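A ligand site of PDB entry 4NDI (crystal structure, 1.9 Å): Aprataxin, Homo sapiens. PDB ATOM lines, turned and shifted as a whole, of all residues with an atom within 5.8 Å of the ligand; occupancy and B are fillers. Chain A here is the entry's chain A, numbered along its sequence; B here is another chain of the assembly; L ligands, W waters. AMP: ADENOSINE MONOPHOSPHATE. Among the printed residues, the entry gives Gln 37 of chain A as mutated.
N of Met 96 is in hydrogen-bond range of O2P of the ligand, 2.9 Å away.
O3P of the ligand is in hydrogen-bond range of NE2 of His 100.
A ring nitrogen (NE2) of His 102 lies within hydrogen-bond range of an oxygen (O3P) of the ligand (2.9 Å).
An oxygen (O2') of the ligand lies close to the backbone carbonyl oxygen of Tyr 35 (3.4 Å).
N3 of the ligand sits at hydrogen-bond distance from N of Lys 34 (3.2 Å).
The side-chain hydroxyl of Ser 14 is in hydrogen-bond range of a nitrogen (N1) of the ligand, at 3.0 Å.
The side-chain carboxylate (OD2) of Asp 33 is in hydrogen-bond range of an oxygen (O3') of the ligand, at 2.5 Å.
O2P of the ligand lies within hydrogen-bond range of N of Ser 95 (2.7 Å).
A ring nitrogen (ND1) of His 91 lies within hydrogen-bond range of an oxygen (O1P) of the ligand, 2.7 Å away.
N of Asp 33 sits at hydrogen-bond distance from O of His 41 (2.9 Å).
OG of Ser 14 sits at hydrogen-bond distance from SD of Met 20 (3.2 Å).
The backbone NH (N) of Lys 32 lies within hydrogen-bond range of the backbone carbonyl oxygen (O) of Met 20, 3.1 Å away.
A ring nitrogen (ND1) of His 102 sits at hydrogen-bond distance from a ring nitrogen (NE2) of His 41 (2.9 Å).
The backbone carbonyl oxygen (O) of Ile 31 lies within hydrogen-bond range of the backbone NH (N) of Leu 43 (2.9 Å).
ND1 of His 41 sits at hydrogen-bond distance from N of Gln 37 (2.9 Å).
OD1 of Asp 33 is in hydrogen-bond range of N of Tyr 35 (2.9 Å).
OG of Ser 95 sits at hydrogen-bond distance from O5' of G 1 of chain B, at 3.5 Å.
Residues that only touch the ligand: G 1 of chain B (3.2 Å), Leu 11 (3.5 Å), Met 20 (3.6 Å), Pro 94 (3.6 Å), Gly 10 (3.7 Å), Leu 43 (3.7 Å), Ile 31 (3.8 Å), Lys 32 (3.8 Å) and His 41 (3.8 Å).
Hydrophobic or aromatic side chains within 4 Å of the ligand: Leu 11, Met 20, Ile 31, Tyr 35, His 41, Leu 43, His 91, Pro 94, Met 96, His 100 and His 102.
Within 4 Å of the ligand: Gly 10, Leu 11, Ser 14, Met 20, Ile 31, Lys 32, Asp 33, Lys 34, Tyr 35, His 41, Leu 43, His 91, Pro 94, Ser 95, Met 96, His 100, His 102 and G 1 of chain B.
The nearest printed residue that does not touch the ligand is Ile 93 (4.5 Å).
Water W5 lies within hydrogen-bond range of O1P of the ligand (2.5 Å), OG of Ser 95 (2.6 Å) and OP2 of G 1 of chain B (2.7 Å).
Water W1 bridges an oxygen (O5') of the ligand and a ring nitrogen (ND1) of His 91.
Water W2 lies within hydrogen-bond range of OP1 of DT 2 of chain B (2.6 Å), O of Tyr 35 (2.8 Å), O2' of the ligand (3.0 Å) and NE2 of Gln 37 (3.1 Å).
Water W4 lies within hydrogen-bond range of the backbone carbonyl oxygen of Gly 10, a nitrogen (N6) of the ligand and the side-chain hydroxyl of Ser 14.
Water W3 lies within hydrogen-bond range of N of His 91 (3.1 Å), O3P of the ligand (3.3 Å) and O of His 100 (3.3 Å).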
ATOM      1  N   TRP A   7      10.086  -3.736  33.722  1.00  0.00           N
ATOM      2  CA  TRP A   7       9.638  -5.010  33.125  1.00  0.00           C
ATOM      3  C   TRP A   7      10.806  -5.937  32.791  1.00  0.00           C
ATOM      4  O   TRP A   7      10.683  -7.154  32.889  1.00  0.00           O
ATOM      5  CB  TRP A   7       8.742  -4.774  31.871  1.00  0.00           C
ATOM      6  CG  TRP A   7       9.459  -4.054  30.716  1.00  0.00           C
ATOM      7  CD1 TRP A   7       9.374  -2.732  30.394  1.00  0.00           C
ATOM      8  CD2 TRP A   7      10.331  -4.657  29.754  1.00  0.00           C
ATOM      9  NE1 TRP A   7      10.153  -2.462  29.282  1.00  0.00           N
ATOM     10  CE2 TRP A   7      10.762  -3.636  28.881  1.00  0.00           C
ATOM     11  CE3 TRP A   7      10.807  -5.967  29.548  1.00  0.00           C
ATOM     12  CZ2 TRP A   7      11.636  -3.865  27.826  1.00  0.00           C
ATOM     13  CZ3 TRP A   7      11.687  -6.196  28.480  1.00  0.00           C
ATOM     14  CH2 TRP A   7      12.090  -5.156  27.648  1.00  0.00           C
ATOM     15  N   GLY A  10      11.958  -8.710  35.358  1.00  0.00           N
ATOM     16  CA  GLY A  10      10.927  -9.616  35.832  1.00  0.00           C
ATOM     17  C   GLY A  10      11.389 -11.030  36.125  1.00  0.00           C
ATOM     18  O   GLY A  10      10.832 -11.682  36.991  1.00  0.00           O
ATOM     19  N   LEU A  11      12.390 -11.524  35.405  1.00  0.00           N
ATOM     20  CA  LEU A  11      12.905 -12.875  35.673  1.00  0.00           C
ATOM     21  C   LEU A  11      13.557 -12.982  37.037  1.00  0.00           C
ATOM     22  O   LEU A  11      13.556 -14.035  37.664  1.00  0.00           O
ATOM     23  CB  LEU A  11      13.937 -13.331  34.634  1.00  0.00           C
ATOM     24  CG  LEU A  11      13.451 -13.428  33.195  1.00  0.00           C
ATOM     25  CD1 LEU A  11      14.562 -13.989  32.313  1.00  0.00           C
ATOM     26  CD2 LEU A  11      12.183 -14.284  33.075  1.00  0.00           C
ATOM     27  N   SER A  14      10.604 -13.713  39.306  1.00  0.00           N
ATOM     28  CA  SER A  14      10.048 -15.043  39.049  1.00  0.00           C
ATOM     29  C   SER A  14      10.940 -16.188  39.479  1.00  0.00           C
ATOM     30  O   SER A  14      10.454 -17.201  39.972  1.00  0.00           O
ATOM     31  CB  SER A  14       9.692 -15.189  37.573  1.00  0.00           C
ATOM     32  OG  SER A  14       8.501 -14.484  37.323  1.00  0.00           O
ATOM     33  N   MET A  20       6.625 -20.792  40.697  1.00  0.00           N
ATOM     34  CA  MET A  20       7.087 -20.854  39.321  1.00  0.00           C
ATOM     35  C   MET A  20       8.273 -21.796  39.180  1.00  0.00           C
ATOM     36  O   MET A  20       8.612 -22.217  38.089  1.00  0.00           O
ATOM     37  CB  MET A  20       7.424 -19.465  38.793  1.00  0.00           C
ATOM     38  CG  MET A  20       6.216 -18.521  38.714  1.00  0.00           C
ATOM     39  SD  MET A  20       6.665 -17.009  37.842  1.00  0.00           S
ATOM     40  CE  MET A  20       6.718 -17.581  36.128  1.00  0.00           C
ATOM     41  N   ILE A  31      12.360 -22.360  35.900  1.00  0.00           N
ATOM     42  CA  ILE A  31      11.011 -21.886  36.075  1.00  0.00           C
ATOM     43  C   ILE A  31      10.195 -22.130  34.807  1.00  0.00           C
ATOM     44  O   ILE A  31      10.755 -22.285  33.718  1.00  0.00           O
ATOM     45  CB  ILE A  31      10.977 -20.370  36.414  1.00  0.00           C
ATOM     46  CG1 ILE A  31      11.617 -19.559  35.280  1.00  0.00           C
ATOM     47  CG2 ILE A  31      11.677 -20.113  37.758  1.00  0.00           C
ATOM     48  CD1 ILE A  31      11.466 -18.029  35.477  1.00  0.00           C
ATOM     49  N   LYS A  32       8.872 -22.167  34.954  1.00  0.00           N
ATOM     50  CA  LYS A  32       8.004 -22.145  33.776  1.00  0.00           C
ATOM     51  C   LYS A  32       8.067 -20.790  33.053  1.00  0.00           C
ATOM     52  O   LYS A  32       8.026 -19.749  33.685  1.00  0.00           O
ATOM     53  CB  LYS A  32       6.566 -22.430  34.195  1.00  0.00           C
ATOM     54  CG  LYS A  32       6.375 -23.852  34.735  1.00  0.00           C
ATOM     55  CD  LYS A  32       4.896 -24.192  34.913  1.00  0.00           C
ATOM     56  CE  LYS A  32       4.318 -23.461  36.085  1.00  0.00           C
ATOM     57  NZ  LYS A  32       2.878 -23.761  36.341  1.00  0.00           N
ATOM     58  N   ASP A  33       8.141 -20.805  31.731  1.00  0.00           N
ATOM     59  CA  ASP A  33       8.072 -19.554  30.988  1.00  0.00           C
ATOM     60  C   ASP A  33       6.675 -18.966  31.184  1.00  0.00           C
ATOM     61  O   ASP A  33       5.677 -19.668  31.062  1.00  0.00           O
ATOM     62  CB  ASP A  33       8.359 -19.792  29.495  1.00  0.00           C
ATOM     63  CG  ASP A  33       8.621 -18.487  28.762  1.00  0.00           C
ATOM     64  OD1 ASP A  33       7.648 -17.741  28.542  1.00  0.00           O
ATOM     65  OD2 ASP A  33       9.789 -18.210  28.409  1.00  0.00           O
ATOM     66  N   LYS A  34       6.607 -17.680  31.525  1.00  0.00           N
ATOM     67  CA  LYS A  34       5.334 -17.048  31.837  1.00  0.00           C
ATOM     68  C   LYS A  34       4.410 -16.920  30.610  1.00  0.00           C
ATOM     69  O   LYS A  34       3.169 -16.922  30.739  1.00  0.00           O
ATOM     70  CB  LYS A  34       5.591 -15.664  32.435  1.00  0.00           C
ATOM     71  CG  LYS A  34       4.329 -14.971  32.972  1.00  0.00           C
ATOM     72  CD  LYS A  34       4.681 -13.670  33.663  1.00  0.00           C
ATOM     73  CE  LYS A  34       3.439 -12.998  34.242  1.00  0.00           C
ATOM     74  NZ  LYS A  34       3.785 -11.636  34.733  1.00  0.00           N
ATOM     75  N   TYR A  35       5.014 -16.814  29.438  1.00  0.00           N
ATOM     76  CA  TYR A  35       4.269 -16.670  28.179  1.00  0.00           C
ATOM     77  C   TYR A  35       4.794 -17.701  27.195  1.00  0.00           C
ATOM     78  O   TYR A  35       5.481 -17.354  26.231  1.00  0.00           O
ATOM     79  CB  TYR A  35       4.457 -15.276  27.596  1.00  0.00           C
ATOM     80  CG  TYR A  35       4.089 -14.175  28.553  1.00  0.00           C
ATOM     81  CD1 TYR A  35       2.763 -13.846  28.773  1.00  0.00           C
ATOM     82  CD2 TYR A  35       5.071 -13.469  29.244  1.00  0.00           C
ATOM     83  CE1 TYR A  35       2.409 -12.830  29.646  1.00  0.00           C
ATOM     84  CE2 TYR A  35       4.733 -12.455  30.133  1.00  0.00           C
ATOM     85  CZ  TYR A  35       3.393 -12.140  30.321  1.00  0.00           C
ATOM     86  OH  TYR A  35       3.038 -11.131  31.201  1.00  0.00           O
ATOM     87  N   PRO A  36       4.504 -18.983  27.466  1.00  0.00           N
ATOM     88  CA  PRO A  36       5.178 -20.086  26.774  1.00  0.00           C
ATOM     89  C   PRO A  36       4.895 -20.096  25.279  1.00  0.00           C
ATOM     90  O   PRO A  36       3.758 -19.794  24.885  1.00  0.00           O
ATOM     91  CB  PRO A  36       4.622 -21.350  27.457  1.00  0.00           C
ATOM     92  CG  PRO A  36       3.347 -20.922  28.109  1.00  0.00           C
ATOM     93  CD  PRO A  36       3.532 -19.469  28.473  1.00  0.00           C
ATOM     94  N   GLN A  37       5.891 -20.453  24.466  1.00  0.00           N
ATOM     95  CA  GLN A  37       5.720 -20.444  23.015  1.00  0.00           C
ATOM     96  C   GLN A  37       5.434 -21.837  22.474  1.00  0.00           C
ATOM     97  O   GLN A  37       5.372 -22.032  21.270  1.00  0.00           O
ATOM     98  CB  GLN A  37       6.956 -19.832  22.338  1.00  0.00           C
ATOM     99  CG  GLN A  37       7.110 -18.338  22.607  1.00  0.00           C
ATOM    100  CD  GLN A  37       6.086 -17.531  21.858  1.00  0.00           C
ATOM    101  OE1 GLN A  37       5.728 -17.881  20.723  1.00  0.00           O
ATOM    102  NE2 GLN A  37       5.586 -16.469  22.472  1.00  0.00           N
ATOM    103  N   HIS A  41       7.724 -25.180  27.919  1.00  0.00           N
ATOM    104  CA  HIS A  41       8.659 -24.083  27.724  1.00  0.00           C
ATOM    105  C   HIS A  41       9.157 -23.665  29.105  1.00  0.00           C
ATOM    106  O   HIS A  41       8.406 -23.081  29.899  1.00  0.00           O
ATOM    107  CB  HIS A  41       7.958 -22.915  26.996  1.00  0.00           C
ATOM    108  CG  HIS A  41       8.889 -21.838  26.517  1.00  0.00           C
ATOM    109  ND1 HIS A  41       8.437 -20.749  25.789  1.00  0.00           N
ATOM    110  CD2 HIS A  41      10.221 -21.662  26.662  1.00  0.00           C
ATOM    111  CE1 HIS A  41       9.465 -19.960  25.500  1.00  0.00           C
ATOM    112  NE2 HIS A  41      10.555 -20.491  26.009  1.00  0.00           N
ATOM    113  N   LEU A  43      12.571 -22.003  31.458  1.00  0.00           N
ATOM    114  CA  LEU A  43      13.799 -21.205  31.467  1.00  0.00           C
ATOM    115  C   LEU A  43      14.688 -21.721  32.575  1.00  0.00           C
ATOM    116  O   LEU A  43      14.211 -21.886  33.700  1.00  0.00           O
ATOM    117  CB  LEU A  43      13.454 -19.747  31.782  1.00  0.00           C
ATOM    118  CG  LEU A  43      12.555 -19.026  30.767  1.00  0.00           C
ATOM    119  CD1 LEU A  43      12.346 -17.562  31.218  1.00  0.00           C
ATOM    120  CD2 LEU A  43      13.127 -19.128  29.343  1.00  0.00           C
ATOM    121  N   HIS A  91      18.235 -16.664  22.984  1.00  0.00           N
ATOM    122  CA  HIS A  91      17.971 -15.605  22.017  1.00  0.00           C
ATOM    123  C   HIS A  91      19.206 -14.734  21.841  1.00  0.00           C
ATOM    124  O   HIS A  91      19.822 -14.312  22.828  1.00  0.00           O
ATOM    125  CB  HIS A  91      16.786 -14.767  22.458  1.00  0.00           C
ATOM    126  CG  HIS A  91      15.464 -15.438  22.197  1.00  0.00           C
ATOM    127  ND1 HIS A  91      14.288 -15.032  22.789  1.00  0.00           N
ATOM    128  CD2 HIS A  91      15.144 -16.488  21.407  1.00  0.00           C
ATOM    129  CE1 HIS A  91      13.299 -15.811  22.371  1.00  0.00           C
ATOM    130  NE2 HIS A  91      13.794 -16.696  21.531  1.00  0.00           N
ATOM    131  N   ILE A  93      19.589 -11.772  20.928  1.00  0.00           N
ATOM    132  CA  ILE A  93      19.361 -10.485  21.584  1.00  0.00           C
ATOM    133  C   ILE A  93      18.168 -10.657  22.506  1.00  0.00           C
ATOM    134  O   ILE A  93      17.018 -10.629  22.060  1.00  0.00           O
ATOM    135  CB  ILE A  93      19.091  -9.334  20.595  1.00  0.00           C
ATOM    136  CG1 ILE A  93      20.263  -9.190  19.596  1.00  0.00           C
ATOM    137  CG2 ILE A  93      18.898  -7.999  21.353  1.00  0.00           C
ATOM    138  CD1 ILE A  93      20.049  -8.110  18.545  1.00  0.00           C
ATOM    139  N   PRO A  94      18.446 -10.850  23.805  1.00  0.00           N
ATOM    140  CA  PRO A  94      17.341 -11.056  24.739  1.00  0.00           C
ATOM    141  C   PRO A  94      16.651  -9.727  25.066  1.00  0.00           C
ATOM    142  O   PRO A  94      17.191  -8.657  24.789  1.00  0.00           O
ATOM    143  CB  PRO A  94      18.054 -11.629  25.984  1.00  0.00           C
ATOM    144  CG  PRO A  94      19.418 -11.049  25.941  1.00  0.00           C
ATOM    145  CD  PRO A  94      19.763 -10.866  24.460  1.00  0.00           C
ATOM    146  N   SER A  95      15.463  -9.814  25.626  1.00  0.00           N
ATOM    147  CA  SER A  95      14.745  -8.659  26.129  1.00  0.00           C
ATOM    148  C   SER A  95      14.856  -8.566  27.674  1.00  0.00           C
ATOM    149  O   SER A  95      14.944  -7.473  28.256  1.00  0.00           O
ATOM    150  CB  SER A  95      13.277  -8.780  25.724  1.00  0.00           C
ATOM    151  OG  SER A  95      13.125  -8.630  24.306  1.00  0.00           O
ATOM    152  N   MET A  96      14.833  -9.727  28.316  1.00  0.00           N
ATOM    153  CA  MET A  96      14.826  -9.798  29.782  1.00  0.00           C
ATOM    154  C   MET A  96      16.239  -9.961  30.305  1.00  0.00           C
ATOM    155  O   MET A  96      17.018 -10.750  29.756  1.00  0.00           O
ATOM    156  CB  MET A  96      13.973 -10.986  30.248  1.00  0.00           C
ATOM    157  CG  MET A  96      12.478 -10.956  29.803  1.00  0.00           C
ATOM    158  SD  MET A  96      11.560  -9.595  30.508  1.00  0.00           S
ATOM    159  CE  MET A  96      11.439 -10.146  32.209  1.00  0.00           C
ATOM    160  N   HIS A 100      19.445 -16.668  30.693  1.00  0.00           N
ATOM    161  CA  HIS A 100      18.447 -17.690  30.850  1.00  0.00           C
ATOM    162  C   HIS A 100      18.453 -18.561  29.617  1.00  0.00           C
ATOM    163  O   HIS A 100      18.495 -18.058  28.503  1.00  0.00           O
ATOM    164  CB  HIS A 100      17.051 -17.082  31.096  1.00  0.00           C
ATOM    165  CG  HIS A 100      16.680 -16.009  30.121  1.00  0.00           C
ATOM    166  ND1 HIS A 100      17.086 -14.686  30.266  1.00  0.00           N
ATOM    167  CD2 HIS A 100      15.905 -16.037  28.997  1.00  0.00           C
ATOM    168  CE1 HIS A 100      16.607 -13.968  29.264  1.00  0.00           C
ATOM    169  NE2 HIS A 100      15.895 -14.764  28.480  1.00  0.00           N
ATOM    170  N   HIS A 102      16.533 -21.144  27.239  1.00  0.00           N
ATOM    171  CA  HIS A 102      15.211 -21.609  26.813  1.00  0.00           C
ATOM    172  C   HIS A 102      15.228 -23.117  26.610  1.00  0.00           C
ATOM    173  O   HIS A 102      16.119 -23.628  25.950  1.00  0.00           O
ATOM    174  CB  HIS A 102      14.781 -20.951  25.497  1.00  0.00           C
ATOM    175  CG  HIS A 102      14.399 -19.519  25.632  1.00  0.00           C
ATOM    176  ND1 HIS A 102      13.092 -19.112  25.835  1.00  0.00           N
ATOM    177  CD2 HIS A 102      15.143 -18.381  25.570  1.00  0.00           C
ATOM    178  CE1 HIS A 102      13.051 -17.792  25.911  1.00  0.00           C
ATOM    179  NE2 HIS A 102      14.278 -17.326  25.751  1.00  0.00           N
ATOM    180  N   PHE A 122      12.505 -18.151  17.502  1.00  0.00           N
ATOM    181  CA  PHE A 122      12.802 -19.557  17.812  1.00  0.00           C
ATOM    182  C   PHE A 122      13.187 -20.389  16.597  1.00  0.00           C
ATOM    183  O   PHE A 122      13.519 -21.567  16.729  1.00  0.00           O
ATOM    184  CB  PHE A 122      11.630 -20.223  18.576  1.00  0.00           C
ATOM    185  CG  PHE A 122      11.484 -19.713  19.974  1.00  0.00           C
ATOM    186  CD1 PHE A 122      12.204 -20.288  21.014  1.00  0.00           C
ATOM    187  CD2 PHE A 122      10.673 -18.627  20.257  1.00  0.00           C
ATOM    188  CE1 PHE A 122      12.104 -19.781  22.332  1.00  0.00           C
ATOM    189  CE2 PHE A 122      10.561 -18.131  21.559  1.00  0.00           C
ATOM    190  CZ  PHE A 122      11.287 -18.706  22.587  1.00  0.00           C
ATOM    191  N   TYR A 126      18.512 -16.431  15.128  1.00  0.00           N
ATOM    192  CA  TYR A 126      18.253 -15.639  16.328  1.00  0.00           C
ATOM    193  C   TYR A 126      18.196 -16.548  17.557  1.00  0.00           C
ATOM    194  O   TYR A 126      18.374 -16.100  18.682  1.00  0.00           O
ATOM    195  CB  TYR A 126      16.902 -14.953  16.185  1.00  0.00           C
ATOM    196  CG  TYR A 126      16.706 -13.707  17.024  1.00  0.00           C
ATOM    197  CD1 TYR A 126      16.185 -13.780  18.306  1.00  0.00           C
ATOM    198  CD2 TYR A 126      16.990 -12.457  16.501  1.00  0.00           C
ATOM    199  CE1 TYR A 126      15.949 -12.626  19.056  1.00  0.00           C
ATOM    200  CE2 TYR A 126      16.767 -11.302  17.226  1.00  0.00           C
ATOM    201  CZ  TYR A 126      16.247 -11.398  18.499  1.00  0.00           C
ATOM    202  OH  TYR A 126      16.024 -10.244  19.224  1.00  0.00           O
ATOM    203  OP3   G B   1       8.545 -11.084  21.978  1.00  0.00           O
ATOM    204  P     G B   1       9.856 -10.211  22.314  1.00  0.00           P
ATOM    205  OP1   G B   1       9.619  -8.817  21.859  1.00  0.00           O
ATOM    206  OP2   G B   1      11.030 -10.923  21.754  1.00  0.00           O
ATOM    207  O5'   G B   1      10.009 -10.109  23.905  1.00  0.00           O
ATOM    208  C5'   G B   1      10.274 -11.240  24.741  1.00  0.00           C
ATOM    209  C4'   G B   1       9.550 -11.071  26.056  1.00  0.00           C
ATOM    210  O4'   G B   1      10.173 -10.006  26.823  1.00  0.00           O
ATOM    211  C3'   G B   1       8.102 -10.632  25.913  1.00  0.00           C
ATOM    212  O3'   G B   1       7.239 -11.731  25.714  1.00  0.00           O
ATOM    213  C2'   G B   1       7.848  -9.873  27.210  1.00  0.00           C
ATOM    214  O2'   G B   1       7.702 -10.775  28.296  1.00  0.00           O
ATOM    215  C1'   G B   1       9.180  -9.178  27.397  1.00  0.00           C
ATOM    216  N9    G B   1       9.263  -7.848  26.739  1.00  0.00           N
ATOM    217  C8    G B   1      10.077  -7.497  25.690  1.00  0.00           C
ATOM    218  N7    G B   1       9.974  -6.237  25.371  1.00  0.00           N
ATOM    219  C5    G B   1       9.062  -5.709  26.276  1.00  0.00           C
ATOM    220  C6    G B   1       8.572  -4.386  26.436  1.00  0.00           C
ATOM    221  O6    G B   1       8.855  -3.370  25.772  1.00  0.00           O
ATOM    222  N1    G B   1       7.659  -4.271  27.480  1.00  0.00           N
ATOM    223  C2    G B   1       7.279  -5.330  28.283  1.00  0.00           C
ATOM    224  N2    G B   1       6.370  -5.039  29.234  1.00  0.00           N
ATOM    225  N3    G B   1       7.737  -6.564  28.151  1.00  0.00           N
ATOM    226  C4    G B   1       8.619  -6.692  27.129  1.00  0.00           C
ATOM    227  P    DT B   2       5.995 -11.601  24.727  1.00  0.00           P
ATOM    228  OP1  DT B   2       5.434 -12.974  24.657  1.00  0.00           O
ATOM    229  OP2  DT B   2       6.399 -10.871  23.488  1.00  0.00           O
ATOM    230  O5'  DT B   2       4.979 -10.620  25.512  1.00  0.00           O
ATOM    231  C5'  DT B   2       4.410 -11.018  26.768  1.00  0.00           C
ATOM    232  C4'  DT B   2       3.669  -9.851  27.396  1.00  0.00           C
ATOM    233  O4'  DT B   2       4.585  -8.739  27.576  1.00  0.00           O
ATOM    234  C3'  DT B   2       2.550  -9.273  26.521  1.00  0.00           C
ATOM    235  O3'  DT B   2       1.336  -9.983  26.781  1.00  0.00           O
ATOM    236  C2'  DT B   2       2.459  -7.846  27.017  1.00  0.00           C
ATOM    237  C1'  DT B   2       3.895  -7.511  27.377  1.00  0.00           C
ATOM    238  N1   DT B   2       4.592  -6.705  26.337  1.00  0.00           N
ATOM    239  C2   DT B   2       4.352  -5.365  26.333  1.00  0.00           C
ATOM    240  O2   DT B   2       3.587  -4.830  27.117  1.00  0.00           O
ATOM    241  N3   DT B   2       5.035  -4.658  25.377  1.00  0.00           N
ATOM    242  C4   DT B   2       5.901  -5.158  24.432  1.00  0.00           C
ATOM    243  O4   DT B   2       6.438  -4.410  23.633  1.00  0.00           O
ATOM    244  C5   DT B   2       6.120  -6.587  24.485  1.00  0.00           C
ATOM    245  C7   DT B   2       7.042  -7.240  23.482  1.00  0.00           C
ATOM    246  C6   DT B   2       5.463  -7.297  25.415  1.00  0.00           C
HETATM  247  P   AMP L   1      14.070 -13.233  25.839  1.00  0.00           P
HETATM  248  O1P AMP L   1      13.916 -12.918  24.372  1.00  0.00           O
HETATM  249  O2P AMP L   1      14.566 -12.132  26.733  1.00  0.00           O
HETATM  250  O3P AMP L   1      14.796 -14.529  26.077  1.00  0.00           O
HETATM  251  O5' AMP L   1      12.565 -13.540  26.220  1.00  0.00           O
HETATM  252  C5' AMP L   1      12.147 -13.556  27.584  1.00  0.00           C
HETATM  253  C4' AMP L   1      11.371 -14.802  27.920  1.00  0.00           C
HETATM  254  O4' AMP L   1      10.939 -14.711  29.289  1.00  0.00           O
HETATM  255  C3' AMP L   1      10.113 -15.002  27.068  1.00  0.00           C
HETATM  256  O3' AMP L   1       9.994 -16.371  26.705  1.00  0.00           O
HETATM  257  C2' AMP L   1       8.970 -14.599  28.014  1.00  0.00           C
HETATM  258  O2' AMP L   1       7.769 -15.293  27.784  1.00  0.00           O
HETATM  259  C1' AMP L   1       9.543 -14.941  29.380  1.00  0.00           C
HETATM  260  N9  AMP L   1       9.083 -14.109  30.492  1.00  0.00           N
HETATM  261  C8  AMP L   1       8.865 -12.776  30.516  1.00  0.00           C
HETATM  262  N7  AMP L   1       8.567 -12.385  31.787  1.00  0.00           N
HETATM  263  C5  AMP L   1       8.618 -13.482  32.583  1.00  0.00           C
HETATM  264  C6  AMP L   1       8.411 -13.787  34.012  1.00  0.00           C
HETATM  265  N6  AMP L   1       8.065 -12.799  34.888  1.00  0.00           N
HETATM  266  N1  AMP L   1       8.572 -15.067  34.409  1.00  0.00           N
HETATM  267  C2  AMP L   1       8.913 -16.054  33.563  1.00  0.00           C
HETATM  268  N3  AMP L   1       9.110 -15.843  32.252  1.00  0.00           N
HETATM  269  C4  AMP L   1       8.982 -14.596  31.727  1.00  0.00           C
HETATM  270  O   HOH W   1      11.143 -14.473  23.821  1.00  0.00           O
HETATM  271  O   HOH W   2       6.781 -15.166  25.003  1.00  0.00           O
HETATM  272  O   HOH W   3      17.654 -16.103  25.956  1.00  0.00           O
HETATM  273  O   HOH W   4       7.956 -11.176  37.385  1.00  0.00           O
HETATM  274  O   HOH W   5      13.316 -10.895  23.124  1.00  0.00           O
HETATM  275  O   HOH W   6       9.141 -16.091  24.066  1.00  0.00           O
